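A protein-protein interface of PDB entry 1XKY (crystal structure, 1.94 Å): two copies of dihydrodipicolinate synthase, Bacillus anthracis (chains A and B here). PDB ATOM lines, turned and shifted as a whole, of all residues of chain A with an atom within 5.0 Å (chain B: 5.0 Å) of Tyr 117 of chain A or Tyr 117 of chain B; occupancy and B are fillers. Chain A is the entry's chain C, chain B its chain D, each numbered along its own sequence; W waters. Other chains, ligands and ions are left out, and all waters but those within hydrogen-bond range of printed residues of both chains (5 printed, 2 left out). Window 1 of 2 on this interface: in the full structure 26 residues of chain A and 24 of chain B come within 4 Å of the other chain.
The guanidinium group of Arg 149 of chain B is in hydrogen-bond range of the backbone carbonyl oxygen of Tyr 118 of chain A, at 2.9 Å.
NH1 of Arg 149 of chain A sits at hydrogen-bond distance from O of Tyr 118 of chain B (2.9 Å).
OD1 of Asn 91 of chain A sits close to O of Tyr 117 of chain A, at 3.0 Å.
The backbone carbonyl oxygen (O) of Asn 91 of chain A is in hydrogen-bond range of the side-chain amide nitrogen (ND2) of Asn 119 of chain A (3.0 Å).
OD1 of Asn 119 of chain A lies close to O of Tyr 117 of chain A, at 3.2 Å.
The side-chain amide oxygen of Asn 91 of chain B sits close to the backbone carbonyl oxygen of Tyr 117 of chain B.
The side-chain amide nitrogen of Asn 119 of chain B lies within hydrogen-bond range of the backbone carbonyl oxygen of Asn 91 of chain B (3.0 Å).
O of Tyr 117 of chain B lies close to OD1 of Asn 119 of chain B, 3.1 Å away.
Among the printed residues, merely in contact across the chains: Val 114 of chain A with Tyr 118 of chain B (3.7 Å), Tyr 117 of chain A with Tyr 117 of chain B (3.8 Å), Tyr 117 of chain A with Tyr 118 of chain B (3.6 Å), Tyr 118 of chain A with Val 114 of chain B (3.8 Å), Tyr 118 of chain A with Tyr 117 of chain B (3.5 Å), Asn 119 of chain A with Arg 149 of chain B (3.7 Å), Lys 120 of chain A with Arg 149 of chain B (3.9 Å) and Arg 149 of chain A with Asn 119 of chain B (3.7 Å).
Tyr 117 of chain A touches just these residues of chain B: Tyr 117 and Tyr 118.
Tyr 117 of chain B touches two residues of chain A.
Printed residues of chain B within 4 Å of Asn 119 of chain A: Arg 149 (3.7 Å).
Of the printed residues of chain B, Lys 120 of chain A touches Arg 149.
Of the printed residues of chain A, Arg 149 of chain B touches Tyr 118 (2.9 Å), Asn 119 (3.7 Å) and Lys 120 (3.9 Å).
Printed residues of chain A within 4 Å of Tyr 118 of chain B: Val 114, Tyr 117 and Arg 149.
Of the printed residues of chain A, Asn 119 of chain B touches Arg 149.
Asn 91 of chain A touches none of the printed residues of chain B.
Pro 116 of chain B touches none of the printed residues of chain A.
Hydrophobic or aromatic side chains of chain A within 4 Å of the printed part of chain B: Val 114, Tyr 117 and Tyr 118.
Among the printed residues, 10 pairs touch across the chains.
Tyr 117 of chain A touches its own counterpart, Tyr 117 of chain B.
Tyr 117 of chain A touches Tyr 118 of chain B, and with the chains exchanged Tyr 118 of chain A touches Tyr 117 of chain B.
Tyr 118 of chain A touches Arg 149 of chain B, and with the chains exchanged Arg 149 of chain A touches Tyr 118 of chain B.
Asn 119 of chain A touches Arg 149 of chain B, and with the chains exchanged Arg 149 of chain A touches Asn 119 of chain B.
Positions printed for both chains: 90, 91, 114, 115, 116, 117, 118, 119, 120, 149 and 150.
Of the 10 pairs that touch across the chains among the printed residues, 9 have their exchanged pair printed and touching as well.
Water W4 bridges the backbone carbonyl oxygen (O) of Asn 119 of chain B (2.7 Å) and the guanidinium group (NH1) of Arg 149 of chain A (3.2 Å).
Water W1 lies within hydrogen-bond range of OD1 of Asn 91 of chain B and OH of Tyr 117 of chain A.
Water W2 lies within hydrogen-bond range of OD1 of Asn 91 of chain A (2.9 Å) and OH of Tyr 117 of chain B (3.2 Å).
Water W3 bridges the backbone carbonyl oxygen of Asn 119 of chain A (3.0 Å) and the guanidinium group of Arg 149 of chain B (3.4 Å).
Water W5 lies within hydrogen-bond range of the side-chain amino group of Lys 120 of chain B and the guanidinium group of Arg 149 of chain A.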
ATOM      1  N   SER A  90      20.611 -12.661  19.301  1.00  0.00           N
ATOM      2  CA  SER A  90      19.346 -13.374  19.467  1.00  0.00           C
ATOM      3  C   SER A  90      19.572 -14.578  20.393  1.00  0.00           C
ATOM      4  O   SER A  90      20.557 -14.617  21.132  1.00  0.00           O
ATOM      5  CB  SER A  90      18.801 -13.797  18.097  1.00  0.00           C
ATOM      6  OG  SER A  90      19.646 -14.749  17.472  1.00  0.00           O
ATOM      7  N   ASN A  91      18.653 -15.537  20.373  1.00  0.00           N
ATOM      8  CA  ASN A  91      18.785 -16.771  21.163  1.00  0.00           C
ATOM      9  C   ASN A  91      19.446 -17.942  20.399  1.00  0.00           C
ATOM     10  O   ASN A  91      19.419 -19.084  20.858  1.00  0.00           O
ATOM     11  CB  ASN A  91      17.421 -17.186  21.757  1.00  0.00           C
ATOM     12  CG  ASN A  91      16.381 -17.603  20.698  1.00  0.00           C
ATOM     13  OD1 ASN A  91      15.279 -18.053  21.050  1.00  0.00           O
ATOM     14  ND2 ASN A  91      16.713 -17.452  19.428  1.00  0.00           N
ATOM     15  N   VAL A 114      21.615  -9.562  23.711  1.00  0.00           N
ATOM     16  CA  VAL A 114      20.686  -9.911  24.783  1.00  0.00           C
ATOM     17  C   VAL A 114      20.889 -11.358  25.270  1.00  0.00           C
ATOM     18  O   VAL A 114      21.294 -12.240  24.500  1.00  0.00           O
ATOM     19  CB  VAL A 114      19.208  -9.668  24.335  1.00  0.00           C
ATOM     20  CG1 VAL A 114      18.738 -10.752  23.358  1.00  0.00           C
ATOM     21  CG2 VAL A 114      18.272  -9.576  25.540  1.00  0.00           C
ATOM     22  N   ALA A 115      20.630 -11.573  26.562  1.00  0.00           N
ATOM     23  CA  ALA A 115      20.475 -12.907  27.113  1.00  0.00           C
ATOM     24  C   ALA A 115      19.440 -13.662  26.289  1.00  0.00           C
ATOM     25  O   ALA A 115      18.329 -13.174  26.119  1.00  0.00           O
ATOM     26  CB  ALA A 115      20.024 -12.835  28.556  1.00  0.00           C
ATOM     27  N   PRO A 116      19.810 -14.838  25.755  1.00  0.00           N
ATOM     28  CA  PRO A 116      18.882 -15.636  24.968  1.00  0.00           C
ATOM     29  C   PRO A 116      17.529 -15.898  25.650  1.00  0.00           C
ATOM     30  O   PRO A 116      17.462 -16.400  26.780  1.00  0.00           O
ATOM     31  CB  PRO A 116      19.649 -16.945  24.752  1.00  0.00           C
ATOM     32  CG  PRO A 116      21.058 -16.530  24.766  1.00  0.00           C
ATOM     33  CD  PRO A 116      21.144 -15.467  25.812  1.00  0.00           C
ATOM     34  N   TYR A 117      16.471 -15.534  24.940  1.00  0.00           N
ATOM     35  CA  TYR A 117      15.101 -15.678  25.401  1.00  0.00           C
ATOM     36  C   TYR A 117      14.610 -17.041  24.940  1.00  0.00           C
ATOM     37  O   TYR A 117      15.212 -17.658  24.056  1.00  0.00           O
ATOM     38  CB  TYR A 117      14.219 -14.556  24.806  1.00  0.00           C
ATOM     39  CG  TYR A 117      14.568 -14.271  23.369  1.00  0.00           C
ATOM     40  CD1 TYR A 117      15.479 -13.262  23.038  1.00  0.00           C
ATOM     41  CD2 TYR A 117      14.048 -15.051  22.338  1.00  0.00           C
ATOM     42  CE1 TYR A 117      15.843 -13.036  21.731  1.00  0.00           C
ATOM     43  CE2 TYR A 117      14.417 -14.828  21.018  1.00  0.00           C
ATOM     44  CZ  TYR A 117      15.316 -13.825  20.727  1.00  0.00           C
ATOM     45  OH  TYR A 117      15.683 -13.586  19.430  1.00  0.00           O
ATOM     46  N   TYR A 118      13.528 -17.496  25.571  1.00  0.00           N
ATOM     47  CA  TYR A 118      12.770 -18.686  25.184  1.00  0.00           C
ATOM     48  C   TYR A 118      13.431 -20.056  25.484  1.00  0.00           C
ATOM     49  O   TYR A 118      12.771 -20.935  26.048  1.00  0.00           O
ATOM     50  CB  TYR A 118      12.321 -18.581  23.724  1.00  0.00           C
ATOM     51  CG  TYR A 118      11.306 -19.619  23.284  1.00  0.00           C
ATOM     52  CD1 TYR A 118      10.137 -19.841  24.008  1.00  0.00           C
ATOM     53  CD2 TYR A 118      11.494 -20.336  22.113  1.00  0.00           C
ATOM     54  CE1 TYR A 118       9.205 -20.782  23.597  1.00  0.00           C
ATOM     55  CE2 TYR A 118      10.571 -21.275  21.686  1.00  0.00           C
ATOM     56  CZ  TYR A 118       9.426 -21.496  22.432  1.00  0.00           C
ATOM     57  OH  TYR A 118       8.512 -22.420  22.006  1.00  0.00           O
ATOM     58  N   ASN A 119      14.699 -20.238  25.125  1.00  0.00           N
ATOM     59  CA  ASN A 119      15.370 -21.538  25.308  1.00  0.00           C
ATOM     60  C   ASN A 119      16.063 -21.754  26.667  1.00  0.00           C
ATOM     61  O   ASN A 119      16.544 -22.858  26.948  1.00  0.00           O
ATOM     62  CB  ASN A 119      16.293 -21.894  24.121  1.00  0.00           C
ATOM     63  CG  ASN A 119      17.314 -20.808  23.768  1.00  0.00           C
ATOM     64  OD1 ASN A 119      17.492 -19.829  24.485  1.00  0.00           O
ATOM     65  ND2 ASN A 119      17.995 -20.996  22.632  1.00  0.00           N
ATOM     66  N   LYS A 120      16.075 -20.718  27.507  1.00  0.00           N
ATOM     67  CA  LYS A 120      16.534 -20.801  28.897  1.00  0.00           C
ATOM     68  C   LYS A 120      17.907 -21.462  29.032  1.00  0.00           C
ATOM     69  O   LYS A 120      18.029 -22.539  29.606  1.00  0.00           O
ATOM     70  CB  LYS A 120      15.502 -21.527  29.767  1.00  0.00           C
ATOM     71  CG  LYS A 120      14.126 -20.867  29.765  1.00  0.00           C
ATOM     72  CD  LYS A 120      13.270 -21.316  30.937  1.00  0.00           C
ATOM     73  CE  LYS A 120      12.840 -22.764  30.811  1.00  0.00           C
ATOM     74  NZ  LYS A 120      12.190 -23.248  32.073  1.00  0.00           N
ATOM     75  N   ARG A 149      12.075 -10.320  30.206  1.00  0.00           N
ATOM     76  CA  ARG A 149      11.757 -10.790  28.850  1.00  0.00           C
ATOM     77  C   ARG A 149      12.377 -12.143  28.473  1.00  0.00           C
ATOM     78  O   ARG A 149      11.798 -12.888  27.672  1.00  0.00           O
ATOM     79  CB  ARG A 149      12.185  -9.747  27.820  1.00  0.00           C
ATOM     80  CG  ARG A 149      11.334  -8.500  27.834  1.00  0.00           C
ATOM     81  CD  ARG A 149      11.823  -7.511  26.807  1.00  0.00           C
ATOM     82  NE  ARG A 149      11.149  -6.219  26.920  1.00  0.00           N
ATOM     83  CZ  ARG A 149       9.994  -5.902  26.335  1.00  0.00           C
ATOM     84  NH1 ARG A 149       9.341  -6.774  25.568  1.00  0.00           N
ATOM     85  NH2 ARG A 149       9.478  -4.695  26.521  1.00  0.00           N
ATOM     86  N   SER A 150      13.558 -12.442  29.014  1.00  0.00           N
ATOM     87  CA  SER A 150      14.293 -13.658  28.644  1.00  0.00           C
ATOM     88  C   SER A 150      14.214 -14.769  29.705  1.00  0.00           C
ATOM     89  O   SER A 150      14.702 -15.872  29.469  1.00  0.00           O
ATOM     90  CB  SER A 150      15.758 -13.312  28.347  1.00  0.00           C
ATOM     91  OG  SER A 150      15.874 -12.522  27.172  1.00  0.00           O
ATOM     92  N   SER B  90       5.924 -18.580  16.097  1.00  0.00           N
ATOM     93  CA  SER B  90       6.972 -17.853  16.804  1.00  0.00           C
ATOM     94  C   SER B  90       6.369 -16.594  17.450  1.00  0.00           C
ATOM     95  O   SER B  90       5.151 -16.505  17.629  1.00  0.00           O
ATOM     96  CB  SER B  90       8.109 -17.523  15.834  1.00  0.00           C
ATOM     97  OG  SER B  90       7.676 -16.675  14.794  1.00  0.00           O
ATOM     98  N   ASN B  91       7.217 -15.631  17.812  1.00  0.00           N
ATOM     99  CA  ASN B  91       6.749 -14.336  18.338  1.00  0.00           C
ATOM    100  C   ASN B  91       6.510 -13.271  17.249  1.00  0.00           C
ATOM    101  O   ASN B  91       6.276 -12.107  17.557  1.00  0.00           O
ATOM    102  CB  ASN B  91       7.681 -13.821  19.452  1.00  0.00           C
ATOM    103  CG  ASN B  91       9.114 -13.549  18.971  1.00  0.00           C
ATOM    104  OD1 ASN B  91       9.936 -13.001  19.720  1.00  0.00           O
ATOM    105  ND2 ASN B  91       9.409 -13.905  17.735  1.00  0.00           N
ATOM    106  N   VAL B 114       2.889 -21.265  19.924  1.00  0.00           N
ATOM    107  CA  VAL B 114       3.280 -20.803  21.239  1.00  0.00           C
ATOM    108  C   VAL B 114       2.883 -19.342  21.469  1.00  0.00           C
ATOM    109  O   VAL B 114       2.866 -18.536  20.537  1.00  0.00           O
ATOM    110  CB  VAL B 114       4.814 -20.981  21.450  1.00  0.00           C
ATOM    111  CG1 VAL B 114       5.619 -19.976  20.626  1.00  0.00           C
ATOM    112  CG2 VAL B 114       5.174 -20.873  22.930  1.00  0.00           C
ATOM    113  N   ALA B 115       2.562 -19.017  22.716  1.00  0.00           N
ATOM    114  CA  ALA B 115       2.470 -17.624  23.155  1.00  0.00           C
ATOM    115  C   ALA B 115       3.768 -16.922  22.769  1.00  0.00           C
ATOM    116  O   ALA B 115       4.845 -17.402  23.118  1.00  0.00           O
ATOM    117  CB  ALA B 115       2.276 -17.550  24.668  1.00  0.00           C
ATOM    118  N   PRO B 116       3.674 -15.801  22.026  1.00  0.00           N
ATOM    119  CA  PRO B 116       4.880 -15.057  21.680  1.00  0.00           C
ATOM    120  C   PRO B 116       5.762 -14.762  22.893  1.00  0.00           C
ATOM    121  O   PRO B 116       5.293 -14.248  23.901  1.00  0.00           O
ATOM    122  CB  PRO B 116       4.326 -13.771  21.049  1.00  0.00           C
ATOM    123  CG  PRO B 116       3.046 -14.195  20.453  1.00  0.00           C
ATOM    124  CD  PRO B 116       2.473 -15.184  21.440  1.00  0.00           C
ATOM    125  N   TYR B 117       7.029 -15.148  22.775  1.00  0.00           N
ATOM    126  CA  TYR B 117       8.049 -14.935  23.801  1.00  0.00           C
ATOM    127  C   TYR B 117       8.739 -13.605  23.506  1.00  0.00           C
ATOM    128  O   TYR B 117       8.640 -13.080  22.396  1.00  0.00           O
ATOM    129  CB  TYR B 117       9.076 -16.086  23.794  1.00  0.00           C
ATOM    130  CG  TYR B 117       9.430 -16.512  22.398  1.00  0.00           C
ATOM    131  CD1 TYR B 117       8.754 -17.562  21.783  1.00  0.00           C
ATOM    132  CD2 TYR B 117      10.386 -15.822  21.661  1.00  0.00           C
ATOM    133  CE1 TYR B 117       9.040 -17.932  20.486  1.00  0.00           C
ATOM    134  CE2 TYR B 117      10.687 -16.190  20.362  1.00  0.00           C
ATOM    135  CZ  TYR B 117      10.002 -17.233  19.782  1.00  0.00           C
ATOM    136  OH  TYR B 117      10.276 -17.600  18.501  1.00  0.00           O
ATOM    137  N   TYR B 118       9.405 -13.068  24.524  1.00  0.00           N
ATOM    138  CA  TYR B 118      10.302 -11.903  24.416  1.00  0.00           C
ATOM    139  C   TYR B 118       9.587 -10.540  24.293  1.00  0.00           C
ATOM    140  O   TYR B 118       9.953  -9.601  24.997  1.00  0.00           O
ATOM    141  CB  TYR B 118      11.342 -12.104  23.291  1.00  0.00           C
ATOM    142  CG  TYR B 118      12.484 -11.098  23.284  1.00  0.00           C
ATOM    143  CD1 TYR B 118      13.249 -10.872  24.423  1.00  0.00           C
ATOM    144  CD2 TYR B 118      12.813 -10.393  22.123  1.00  0.00           C
ATOM    145  CE1 TYR B 118      14.285  -9.943  24.423  1.00  0.00           C
ATOM    146  CE2 TYR B 118      13.856  -9.466  22.110  1.00  0.00           C
ATOM    147  CZ  TYR B 118      14.584  -9.250  23.268  1.00  0.00           C
ATOM    148  OH  TYR B 118      15.622  -8.353  23.270  1.00  0.00           O
ATOM    149  N   ASN B 119       8.592 -10.433  23.409  1.00  0.00           N
ATOM    150  CA  ASN B 119       7.929  -9.149  23.159  1.00  0.00           C
ATOM    151  C   ASN B 119       6.700  -8.872  24.038  1.00  0.00           C
ATOM    152  O   ASN B 119       6.109  -7.792  23.939  1.00  0.00           O
ATOM    153  CB  ASN B 119       7.626  -8.921  21.652  1.00  0.00           C
ATOM    154  CG  ASN B 119       6.903 -10.094  20.967  1.00  0.00           C
ATOM    155  OD1 ASN B 119       6.455 -11.056  21.601  1.00  0.00           O
ATOM    156  ND2 ASN B 119       6.811 -10.011  19.640  1.00  0.00           N
ATOM    157  N   LYS B 120       6.331  -9.838  24.883  1.00  0.00           N
ATOM    158  CA  LYS B 120       5.320  -9.666  25.920  1.00  0.00           C
ATOM    159  C   LYS B 120       4.010  -9.045  25.418  1.00  0.00           C
ATOM    160  O   LYS B 120       3.614  -7.955  25.861  1.00  0.00           O
ATOM    161  CB  LYS B 120       5.880  -8.840  27.083  1.00  0.00           C
ATOM    162  CG  LYS B 120       7.097  -9.457  27.757  1.00  0.00           C
ATOM    163  CD  LYS B 120       7.243  -8.970  29.180  1.00  0.00           C
ATOM    164  CE  LYS B 120       7.695  -7.529  29.248  1.00  0.00           C
ATOM    165  NZ  LYS B 120       7.696  -7.070  30.660  1.00  0.00           N
ATOM    166  N   ARG B 149       8.524 -19.878  29.752  1.00  0.00           N
ATOM    167  CA  ARG B 149       9.405 -19.451  28.651  1.00  0.00           C
ATOM    168  C   ARG B 149       9.008 -18.127  27.967  1.00  0.00           C
ATOM    169  O   ARG B 149       9.871 -17.410  27.474  1.00  0.00           O
ATOM    170  CB  ARG B 149       9.506 -20.547  27.587  1.00  0.00           C
ATOM    171  CG  ARG B 149      10.046 -21.856  28.095  1.00  0.00           C
ATOM    172  CD  ARG B 149      10.134 -22.877  26.968  1.00  0.00           C
ATOM    173  NE  ARG B 149      10.659 -24.154  27.441  1.00  0.00           N
ATOM    174  CZ  ARG B 149      11.949 -24.495  27.473  1.00  0.00           C
ATOM    175  NH1 ARG B 149      12.904 -23.666  27.065  1.00  0.00           N
ATOM    176  NH2 ARG B 149      12.286 -25.691  27.928  1.00  0.00           N
ATOM    177  N   SER B 150       7.717 -17.812  27.923  1.00  0.00           N
ATOM    178  CA  SER B 150       7.242 -16.599  27.240  1.00  0.00           C
ATOM    179  C   SER B 150       6.842 -15.481  28.188  1.00  0.00           C
ATOM    180  O   SER B 150       6.508 -14.388  27.731  1.00  0.00           O
ATOM    181  CB  SER B 150       6.075 -16.940  26.314  1.00  0.00           C
ATOM    182  OG  SER B 150       6.499 -17.837  25.315  1.00  0.00           O
HETATM  183  O   HOH W   1      12.653 -12.486  18.781  1.00  0.00           O
HETATM  184  O   HOH W   2      13.207 -18.713  19.086  1.00  0.00           O
HETATM  185  O   HOH W   3      15.588 -25.314  28.461  1.00  0.00           O
HETATM  186  O   HOH W   4       7.688  -5.786  23.050  1.00  0.00           O
HETATM  187  O   HOH W   5       8.313  -4.171  29.579  1.00  0.00           O
